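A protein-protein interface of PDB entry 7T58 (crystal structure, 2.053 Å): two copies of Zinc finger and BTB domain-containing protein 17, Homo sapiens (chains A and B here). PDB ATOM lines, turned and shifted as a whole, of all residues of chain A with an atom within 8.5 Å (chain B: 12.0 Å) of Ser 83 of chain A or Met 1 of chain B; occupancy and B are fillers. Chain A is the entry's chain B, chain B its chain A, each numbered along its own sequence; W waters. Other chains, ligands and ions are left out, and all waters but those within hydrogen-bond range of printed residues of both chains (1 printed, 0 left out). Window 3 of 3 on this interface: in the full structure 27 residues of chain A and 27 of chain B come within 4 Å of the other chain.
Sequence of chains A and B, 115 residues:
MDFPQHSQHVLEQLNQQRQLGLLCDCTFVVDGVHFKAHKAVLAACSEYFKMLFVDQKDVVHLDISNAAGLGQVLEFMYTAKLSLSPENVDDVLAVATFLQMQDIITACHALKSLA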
ATOM      1  N   ALA A  68       9.205  11.791 -11.530  1.00  0.00           N
ATOM      2  CA  ALA A  68       8.971  13.163 -11.096  1.00  0.00           C
ATOM      3  C   ALA A  68      10.109  14.075 -11.530  1.00  0.00           C
ATOM      4  O   ALA A  68       9.873  15.194 -12.001  1.00  0.00           O
ATOM      5  CB  ALA A  68       8.789  13.214  -9.578  1.00  0.00           C
ATOM      6  N   GLN A  72      10.078  17.237 -14.266  1.00  0.00           N
ATOM      7  CA  GLN A  72      10.586  18.580 -14.010  1.00  0.00           C
ATOM      8  C   GLN A  72      11.591  19.003 -15.074  1.00  0.00           C
ATOM      9  O   GLN A  72      11.599  20.164 -15.499  1.00  0.00           O
ATOM     10  CB  GLN A  72      11.213  18.651 -12.618  1.00  0.00           C
ATOM     11  CG  GLN A  72      10.230  18.413 -11.479  1.00  0.00           C
ATOM     12  CD  GLN A  72      10.869  18.569 -10.113  1.00  0.00           C
ATOM     13  OE1 GLN A  72      11.271  19.668  -9.723  1.00  0.00           O
ATOM     14  NE2 GLN A  72      10.975  17.468  -9.379  1.00  0.00           N
ATOM     15  N   VAL A  73      12.442  18.076 -15.518  1.00  0.00           N
ATOM     16  CA  VAL A  73      13.426  18.406 -16.547  1.00  0.00           C
ATOM     17  C   VAL A  73      12.730  18.705 -17.869  1.00  0.00           C
ATOM     18  O   VAL A  73      13.050  19.689 -18.547  1.00  0.00           O
ATOM     19  CB  VAL A  73      14.454  17.272 -16.692  1.00  0.00           C
ATOM     20  CG1 VAL A  73      15.332  17.508 -17.906  1.00  0.00           C
ATOM     21  CG2 VAL A  73      15.303  17.165 -15.436  1.00  0.00           C
ATOM     22  N   GLU A  75       9.670  19.741 -18.230  1.00  0.00           N
ATOM     23  CA  GLU A  75       9.009  21.026 -18.035  1.00  0.00           C
ATOM     24  C   GLU A  75       9.983  22.180 -18.234  1.00  0.00           C
ATOM     25  O   GLU A  75       9.629  23.207 -18.825  1.00  0.00           O
ATOM     26  CB  GLU A  75       8.381  21.081 -16.641  1.00  0.00           C
ATOM     27  CG  GLU A  75       7.949  22.467 -16.181  1.00  0.00           C
ATOM     28  CD  GLU A  75       6.641  22.918 -16.805  1.00  0.00           C
ATOM     29  OE1 GLU A  75       6.059  22.152 -17.602  1.00  0.00           O
ATOM     30  OE2 GLU A  75       6.192  24.042 -16.492  1.00  0.00           O
ATOM     31  N   PHE A  76      11.219  22.024 -17.753  1.00  0.00           N
ATOM     32  CA  PHE A  76      12.218  23.071 -17.936  1.00  0.00           C
ATOM     33  C   PHE A  76      12.538  23.282 -19.410  1.00  0.00           C
ATOM     34  O   PHE A  76      12.662  24.424 -19.866  1.00  0.00           O
ATOM     35  CB  PHE A  76      13.489  22.729 -17.162  1.00  0.00           C
ATOM     36  CG  PHE A  76      14.709  23.433 -17.678  1.00  0.00           C
ATOM     37  CD1 PHE A  76      14.959  24.751 -17.339  1.00  0.00           C
ATOM     38  CD2 PHE A  76      15.597  22.781 -18.518  1.00  0.00           C
ATOM     39  CE1 PHE A  76      16.077  25.399 -17.822  1.00  0.00           C
ATOM     40  CE2 PHE A  76      16.710  23.425 -19.004  1.00  0.00           C
ATOM     41  CZ  PHE A  76      16.951  24.734 -18.656  1.00  0.00           C
ATOM     42  N   THR A  79       9.662  25.331 -20.782  1.00  0.00           N
ATOM     43  CA  THR A  79       9.216  26.528 -20.074  1.00  0.00           C
ATOM     44  C   THR A  79      10.338  27.389 -19.520  1.00  0.00           C
ATOM     45  O   THR A  79      10.069  28.540 -19.154  1.00  0.00           O
ATOM     46  CB  THR A  79       8.294  26.160 -18.900  1.00  0.00           C
ATOM     47  OG1 THR A  79       9.053  25.455 -17.909  1.00  0.00           O
ATOM     48  CG2 THR A  79       7.125  25.295 -19.361  1.00  0.00           C
ATOM     49  N   ALA A  80      11.566  26.875 -19.428  1.00  0.00           N
ATOM     50  CA  ALA A  80      12.713  27.516 -18.785  1.00  0.00           C
ATOM     51  C   ALA A  80      12.534  27.670 -17.281  1.00  0.00           C
ATOM     52  O   ALA A  80      13.303  28.401 -16.645  1.00  0.00           O
ATOM     53  CB  ALA A  80      13.037  28.883 -19.405  1.00  0.00           C
ATOM     54  N   LYS A  81      11.553  26.995 -16.689  1.00  0.00           N
ATOM     55  CA  LYS A  81      11.302  27.070 -15.257  1.00  0.00           C
ATOM     56  C   LYS A  81      11.720  25.764 -14.592  1.00  0.00           C
ATOM     57  O   LYS A  81      11.538  24.679 -15.154  1.00  0.00           O
ATOM     58  CB  LYS A  81       9.824  27.388 -14.980  1.00  0.00           C
ATOM     59  CG  LYS A  81       8.993  26.251 -14.395  1.00  0.00           C
ATOM     60  CD  LYS A  81       8.804  26.418 -12.894  1.00  0.00           C
ATOM     61  CE  LYS A  81       7.731  25.480 -12.355  1.00  0.00           C
ATOM     62  NZ  LYS A  81       8.083  24.042 -12.526  1.00  0.00           N
ATOM     63  N   LEU A  82      12.301  25.877 -13.400  1.00  0.00           N
ATOM     64  CA  LEU A  82      12.816  24.718 -12.678  1.00  0.00           C
ATOM     65  C   LEU A  82      12.717  24.996 -11.186  1.00  0.00           C
ATOM     66  O   LEU A  82      13.361  25.923 -10.686  1.00  0.00           O
ATOM     67  CB  LEU A  82      14.263  24.426 -13.083  1.00  0.00           C
ATOM     68  CG  LEU A  82      14.957  23.221 -12.445  1.00  0.00           C
ATOM     69  CD1 LEU A  82      14.332  21.926 -12.928  1.00  0.00           C
ATOM     70  CD2 LEU A  82      16.452  23.244 -12.743  1.00  0.00           C
ATOM     71  N   SER A  83      11.915  24.201 -10.481  1.00  0.00           N
ATOM     72  CA  SER A  83      11.694  24.374  -9.046  1.00  0.00           C
ATOM     73  C   SER A  83      12.486  23.302  -8.305  1.00  0.00           C
ATOM     74  O   SER A  83      12.038  22.161  -8.173  1.00  0.00           O
ATOM     75  CB  SER A  83      10.206  24.304  -8.713  1.00  0.00           C
ATOM     76  OG  SER A  83       9.525  25.458  -9.174  1.00  0.00           O
ATOM     77  N   LEU A  84      13.664  23.677  -7.814  1.00  0.00           N
ATOM     78  CA  LEU A  84      14.549  22.763  -7.105  1.00  0.00           C
ATOM     79  C   LEU A  84      14.406  22.956  -5.602  1.00  0.00           C
ATOM     80  O   LEU A  84      14.518  24.080  -5.102  1.00  0.00           O
ATOM     81  CB  LEU A  84      16.005  22.982  -7.518  1.00  0.00           C
ATOM     82  CG  LEU A  84      16.397  22.697  -8.966  1.00  0.00           C
ATOM     83  CD1 LEU A  84      17.875  22.999  -9.168  1.00  0.00           C
ATOM     84  CD2 LEU A  84      16.079  21.253  -9.341  1.00  0.00           C
ATOM     85  N   SER A  85      14.162  21.864  -4.892  1.00  0.00           N
ATOM     86  CA  SER A  85      14.135  21.830  -3.440  1.00  0.00           C
ATOM     87  C   SER A  85      15.179  20.841  -2.941  1.00  0.00           C
ATOM     88  O   SER A  85      15.662  19.998  -3.708  1.00  0.00           O
ATOM     89  CB  SER A  85      12.747  21.423  -2.925  1.00  0.00           C
ATOM     90  OG  SER A  85      12.423  20.107  -3.337  1.00  0.00           O
ATOM     91  N   PRO A  86      15.564  20.920  -1.665  1.00  0.00           N
ATOM     92  CA  PRO A  86      16.432  19.871  -1.105  1.00  0.00           C
ATOM     93  C   PRO A  86      15.842  18.478  -1.218  1.00  0.00           C
ATOM     94  O   PRO A  86      16.592  17.496  -1.144  1.00  0.00           O
ATOM     95  CB  PRO A  86      16.594  20.296   0.361  1.00  0.00           C
ATOM     96  CG  PRO A  86      16.408  21.772   0.339  1.00  0.00           C
ATOM     97  CD  PRO A  86      15.385  22.046  -0.730  1.00  0.00           C
ATOM     98  N   GLU A  87      14.526  18.359  -1.411  1.00  0.00           N
ATOM     99  CA  GLU A  87      13.896  17.050  -1.527  1.00  0.00           C
ATOM    100  C   GLU A  87      13.990  16.473  -2.934  1.00  0.00           C
ATOM    101  O   GLU A  87      13.966  15.248  -3.091  1.00  0.00           O
ATOM    102  CB  GLU A  87      12.426  17.126  -1.107  1.00  0.00           C
ATOM    103  CG  GLU A  87      12.197  17.141   0.395  1.00  0.00           C
ATOM    104  CD  GLU A  87      10.729  16.996   0.757  1.00  0.00           C
ATOM    105  OE1 GLU A  87      10.052  16.124   0.167  1.00  0.00           O
ATOM    106  OE2 GLU A  87      10.248  17.758   1.624  1.00  0.00           O
ATOM    107  N   ASN A  88      14.085  17.317  -3.965  1.00  0.00           N
ATOM    108  CA  ASN A  88      14.095  16.829  -5.339  1.00  0.00           C
ATOM    109  C   ASN A  88      15.420  17.031  -6.059  1.00  0.00           C
ATOM    110  O   ASN A  88      15.579  16.519  -7.174  1.00  0.00           O
ATOM    111  CB  ASN A  88      12.964  17.486  -6.156  1.00  0.00           C
ATOM    112  CG  ASN A  88      13.155  18.991  -6.359  1.00  0.00           C
ATOM    113  OD1 ASN A  88      14.261  19.527  -6.244  1.00  0.00           O
ATOM    114  ND2 ASN A  88      12.063  19.677  -6.674  1.00  0.00           N
ATOM    115  N   VAL A  89      16.366  17.764  -5.466  1.00  0.00           N
ATOM    116  CA  VAL A  89      17.567  18.152  -6.202  1.00  0.00           C
ATOM    117  C   VAL A  89      18.387  16.925  -6.580  1.00  0.00           C
ATOM    118  O   VAL A  89      18.992  16.873  -7.659  1.00  0.00           O
ATOM    119  CB  VAL A  89      18.390  19.171  -5.390  1.00  0.00           C
ATOM    120  CG1 VAL A  89      18.867  18.565  -4.070  1.00  0.00           C
ATOM    121  CG2 VAL A  89      19.566  19.684  -6.215  1.00  0.00           C
ATOM    122  N   VAL A  92      16.621  15.429  -9.642  1.00  0.00           N
ATOM    123  CA  VAL A  92      16.790  16.209 -10.863  1.00  0.00           C
ATOM    124  C   VAL A  92      18.228  16.121 -11.364  1.00  0.00           C
ATOM    125  O   VAL A  92      18.469  16.019 -12.572  1.00  0.00           O
ATOM    126  CB  VAL A  92      16.348  17.663 -10.622  1.00  0.00           C
ATOM    127  CG1 VAL A  92      16.658  18.521 -11.827  1.00  0.00           C
ATOM    128  CG2 VAL A  92      14.860  17.710 -10.309  1.00  0.00           C
ATOM    129  N   ALA A 107      22.842  24.192 -11.878  1.00  0.00           N
ATOM    130  CA  ALA A 107      21.855  24.704 -10.932  1.00  0.00           C
ATOM    131  C   ALA A 107      21.638  23.750  -9.765  1.00  0.00           C
ATOM    132  O   ALA A 107      21.248  24.187  -8.676  1.00  0.00           O
ATOM    133  CB  ALA A 107      20.532  24.975 -11.650  1.00  0.00           C
ATOM    134  N   LEU A 111      22.612  24.765  -5.577  1.00  0.00           N
ATOM    135  CA  LEU A 111      21.695  24.602  -4.453  1.00  0.00           C
ATOM    136  C   LEU A 111      22.289  23.693  -3.383  1.00  0.00           C
ATOM    137  O   LEU A 111      22.163  23.966  -2.183  1.00  0.00           O
ATOM    138  CB  LEU A 111      20.357  24.053  -4.946  1.00  0.00           C
ATOM    139  CG  LEU A 111      19.334  23.693  -3.865  1.00  0.00           C
ATOM    140  CD1 LEU A 111      18.975  24.918  -3.039  1.00  0.00           C
ATOM    141  CD2 LEU A 111      18.088  23.077  -4.483  1.00  0.00           C
ATOM    142  N   MET B   1      15.748  29.652 -10.700  1.00  0.00           N
ATOM    143  CA  MET B   1      14.460  29.130 -11.141  1.00  0.00           C
ATOM    144  C   MET B   1      14.220  29.380 -12.627  1.00  0.00           C
ATOM    145  O   MET B   1      13.706  28.513 -13.332  1.00  0.00           O
ATOM    146  CB  MET B   1      13.318  29.747 -10.331  1.00  0.00           C
ATOM    147  CG  MET B   1      12.659  28.791  -9.356  1.00  0.00           C
ATOM    148  SD  MET B   1      10.964  29.265  -8.963  1.00  0.00           S
ATOM    149  CE  MET B   1      10.161  29.026 -10.547  1.00  0.00           C
ATOM    150  N   ASP B   2      14.586  30.568 -13.100  1.00  0.00           N
ATOM    151  CA  ASP B   2      14.354  30.961 -14.482  1.00  0.00           C
ATOM    152  C   ASP B   2      15.675  31.116 -15.223  1.00  0.00           C
ATOM    153  O   ASP B   2      16.673  31.573 -14.656  1.00  0.00           O
ATOM    154  CB  ASP B   2      13.564  32.269 -14.566  1.00  0.00           C
ATOM    155  CG  ASP B   2      13.289  32.689 -15.999  1.00  0.00           C
ATOM    156  OD1 ASP B   2      12.493  32.005 -16.678  1.00  0.00           O
ATOM    157  OD2 ASP B   2      13.876  33.694 -16.452  1.00  0.00           O
ATOM    158  N   PHE B   3      15.664  30.734 -16.497  1.00  0.00           N
ATOM    159  CA  PHE B   3      16.821  30.853 -17.384  1.00  0.00           C
ATOM    160  C   PHE B   3      16.430  31.778 -18.527  1.00  0.00           C
ATOM    161  O   PHE B   3      15.769  31.339 -19.487  1.00  0.00           O
ATOM    162  CB  PHE B   3      17.251  29.483 -17.904  1.00  0.00           C
ATOM    163  CG  PHE B   3      17.761  28.553 -16.832  1.00  0.00           C
ATOM    164  CD1 PHE B   3      16.900  28.014 -15.890  1.00  0.00           C
ATOM    165  CD2 PHE B   3      19.103  28.213 -16.774  1.00  0.00           C
ATOM    166  CE1 PHE B   3      17.367  27.159 -14.906  1.00  0.00           C
ATOM    167  CE2 PHE B   3      19.576  27.356 -15.794  1.00  0.00           C
ATOM    168  CZ  PHE B   3      18.706  26.830 -14.859  1.00  0.00           C
ATOM    169  N   PRO B   4      16.811  33.056 -18.478  1.00  0.00           N
ATOM    170  CA  PRO B   4      16.199  34.045 -19.383  1.00  0.00           C
ATOM    171  C   PRO B   4      16.494  33.820 -20.855  1.00  0.00           C
ATOM    172  O   PRO B   4      15.717  34.282 -21.700  1.00  0.00           O
ATOM    173  CB  PRO B   4      16.785  35.376 -18.895  1.00  0.00           C
ATOM    174  CG  PRO B   4      18.072  34.997 -18.234  1.00  0.00           C
ATOM    175  CD  PRO B   4      17.829  33.657 -17.601  1.00  0.00           C
ATOM    176  N   GLN B   5      17.579  33.128 -21.197  1.00  0.00           N
ATOM    177  CA  GLN B   5      17.962  32.931 -22.588  1.00  0.00           C
ATOM    178  C   GLN B   5      17.633  31.534 -23.101  1.00  0.00           C
ATOM    179  O   GLN B   5      18.101  31.158 -24.180  1.00  0.00           O
ATOM    180  CB  GLN B   5      19.454  33.213 -22.765  1.00  0.00           C
ATOM    181  CG  GLN B   5      19.845  34.665 -22.539  1.00  0.00           C
ATOM    182  CD  GLN B   5      21.345  34.859 -22.476  1.00  0.00           C
ATOM    183  OE1 GLN B   5      22.077  33.976 -22.026  1.00  0.00           O
ATOM    184  NE2 GLN B   5      21.814  36.016 -22.933  1.00  0.00           N
ATOM    185  N   HIS B   6      16.835  30.763 -22.359  1.00  0.00           N
ATOM    186  CA  HIS B   6      16.551  29.388 -22.759  1.00  0.00           C
ATOM    187  C   HIS B   6      15.777  29.340 -24.072  1.00  0.00           C
ATOM    188  O   HIS B   6      16.126  28.578 -24.981  1.00  0.00           O
ATOM    189  CB  HIS B   6      15.781  28.667 -21.651  1.00  0.00           C
ATOM    190  CG  HIS B   6      15.404  27.260 -21.996  1.00  0.00           C
ATOM    191  ND1 HIS B   6      16.328  26.239 -22.069  1.00  0.00           N
ATOM    192  CD2 HIS B   6      14.206  26.704 -22.296  1.00  0.00           C
ATOM    193  CE1 HIS B   6      15.716  25.115 -22.394  1.00  0.00           C
ATOM    194  NE2 HIS B   6      14.428  25.370 -22.538  1.00  0.00           N
ATOM    195  N   SER B   7      14.719  30.150 -24.191  1.00  0.00           N
ATOM    196  CA  SER B   7      13.877  30.088 -25.383  1.00  0.00           C
ATOM    197  C   SER B   7      14.642  30.524 -26.628  1.00  0.00           C
ATOM    198  O   SER B   7      14.459  29.950 -27.707  1.00  0.00           O
ATOM    199  CB  SER B   7      12.628  30.947 -25.195  1.00  0.00           C
ATOM    200  OG  SER B   7      12.939  32.326 -25.280  1.00  0.00           O
HETATM  201  O   HOH W   1       9.685  31.328 -17.793  1.00  0.00           O
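O of Met 1 of chain B sits at hydrogen-bond distance from N of Leu 82 of chain A (3.0 Å). The backbone NH of Phe 3 of chain B lies within hydrogen-bond range of the backbone carbonyl oxygen of Ala 80 of chain A, at 3.3 Å. A ring nitrogen (NE2) of His 6 of chain B is in hydrogen-bond range of the backbone carbonyl oxygen (O) of Phe 76 of chain A. O of Met 1 of chain B lies close to O of Ala 80 of chain A (3.3 Å).
The side-chain amide oxygen (OE1) of Gln 72 of chain A lies close to the backbone carbonyl oxygen (O) of Ser 83 of chain A. The backbone NH of Lys 81 of chain A sits close to the side-chain hydroxyl of Thr 79 of chain A (3.2 Å). The backbone carbonyl oxygen (O) of Ser 83 of chain A is in hydrogen-bond range of the side-chain amide nitrogen (ND2) of Asn 88 of chain A (2.9 Å).
CE1 of Phe 76 of chain A touches CD1 of Phe 3 of chain B, 3.4 Å away. Ala 80 of chain A touches Asp 2 of chain B. CB of Ala 80 of chain A touches CB of His 6 of chain B, 3.6 Å away. CA of Lys 81 of chain A touches O of Met 1 of chain B, 3.4 Å away. Ser 83 of chain A touches Met 1 of chain B.
Glu 75 of chain A touches none of the printed residues of chain B. Of the printed residues of chain B, Phe 76 of chain A touches Phe 3 (3.4 Å) and His 6 (3.3 Å). Of chain B, only Met 1 (3.3 Å), Asp 2 (3.5 Å), Phe 3 (3.3 Å) and His 6 (3.6 Å) come within 4 Å of Ala 80 of chain A. Of chain B, only Met 1 comes within 4 Å of Lys 81 of chain A. Ser 83 of chain A touches just one residue of chain B: Met 1 (3.9 Å). No residue of chain B comes within 4 Å of Leu 84 of chain A. Met 1 of chain B touches four residues of chain A. Printed residues of chain A within 4 Å of Asp 2 of chain B: Ala 80 (3.5 Å). Printed residues of chain A within 4 Å of Phe 3 of chain B: Phe 76 and Ala 80. Of the printed residues of chain A, His 6 of chain B touches Phe 76 and Ala 80. The nearest residue of chain B that does not touch Ser 83 of chain A is Asp 2 of chain B (7.4 Å).
Hydrophobic or aromatic side chains of chain A within 4 Å of the printed part of chain B: Phe 76 and Ala 80. Of the 7 printed residues of chain B, 4 touch a printed residue of chain A. Hydrophobic or aromatic side chains of chain B within 4 Å of the printed part of chain A: Met 1, Phe 3 and His 6. Along chain B the printed residues that touch a printed residue of chain A span positions 1 to 6. Among the printed residues, no Asp or Glu carboxylate lies within 4 Å of a Lys or Arg side-chain nitrogen of the other chain.
No position is printed for both chains. Of the 9 pairs that touch across the chains among the printed residues, none has its exchanged pair printed and touching as well.
Water W1 lies within hydrogen-bond range of OD1 of Asp 2 of chain B and O of Thr 79 of chain A.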
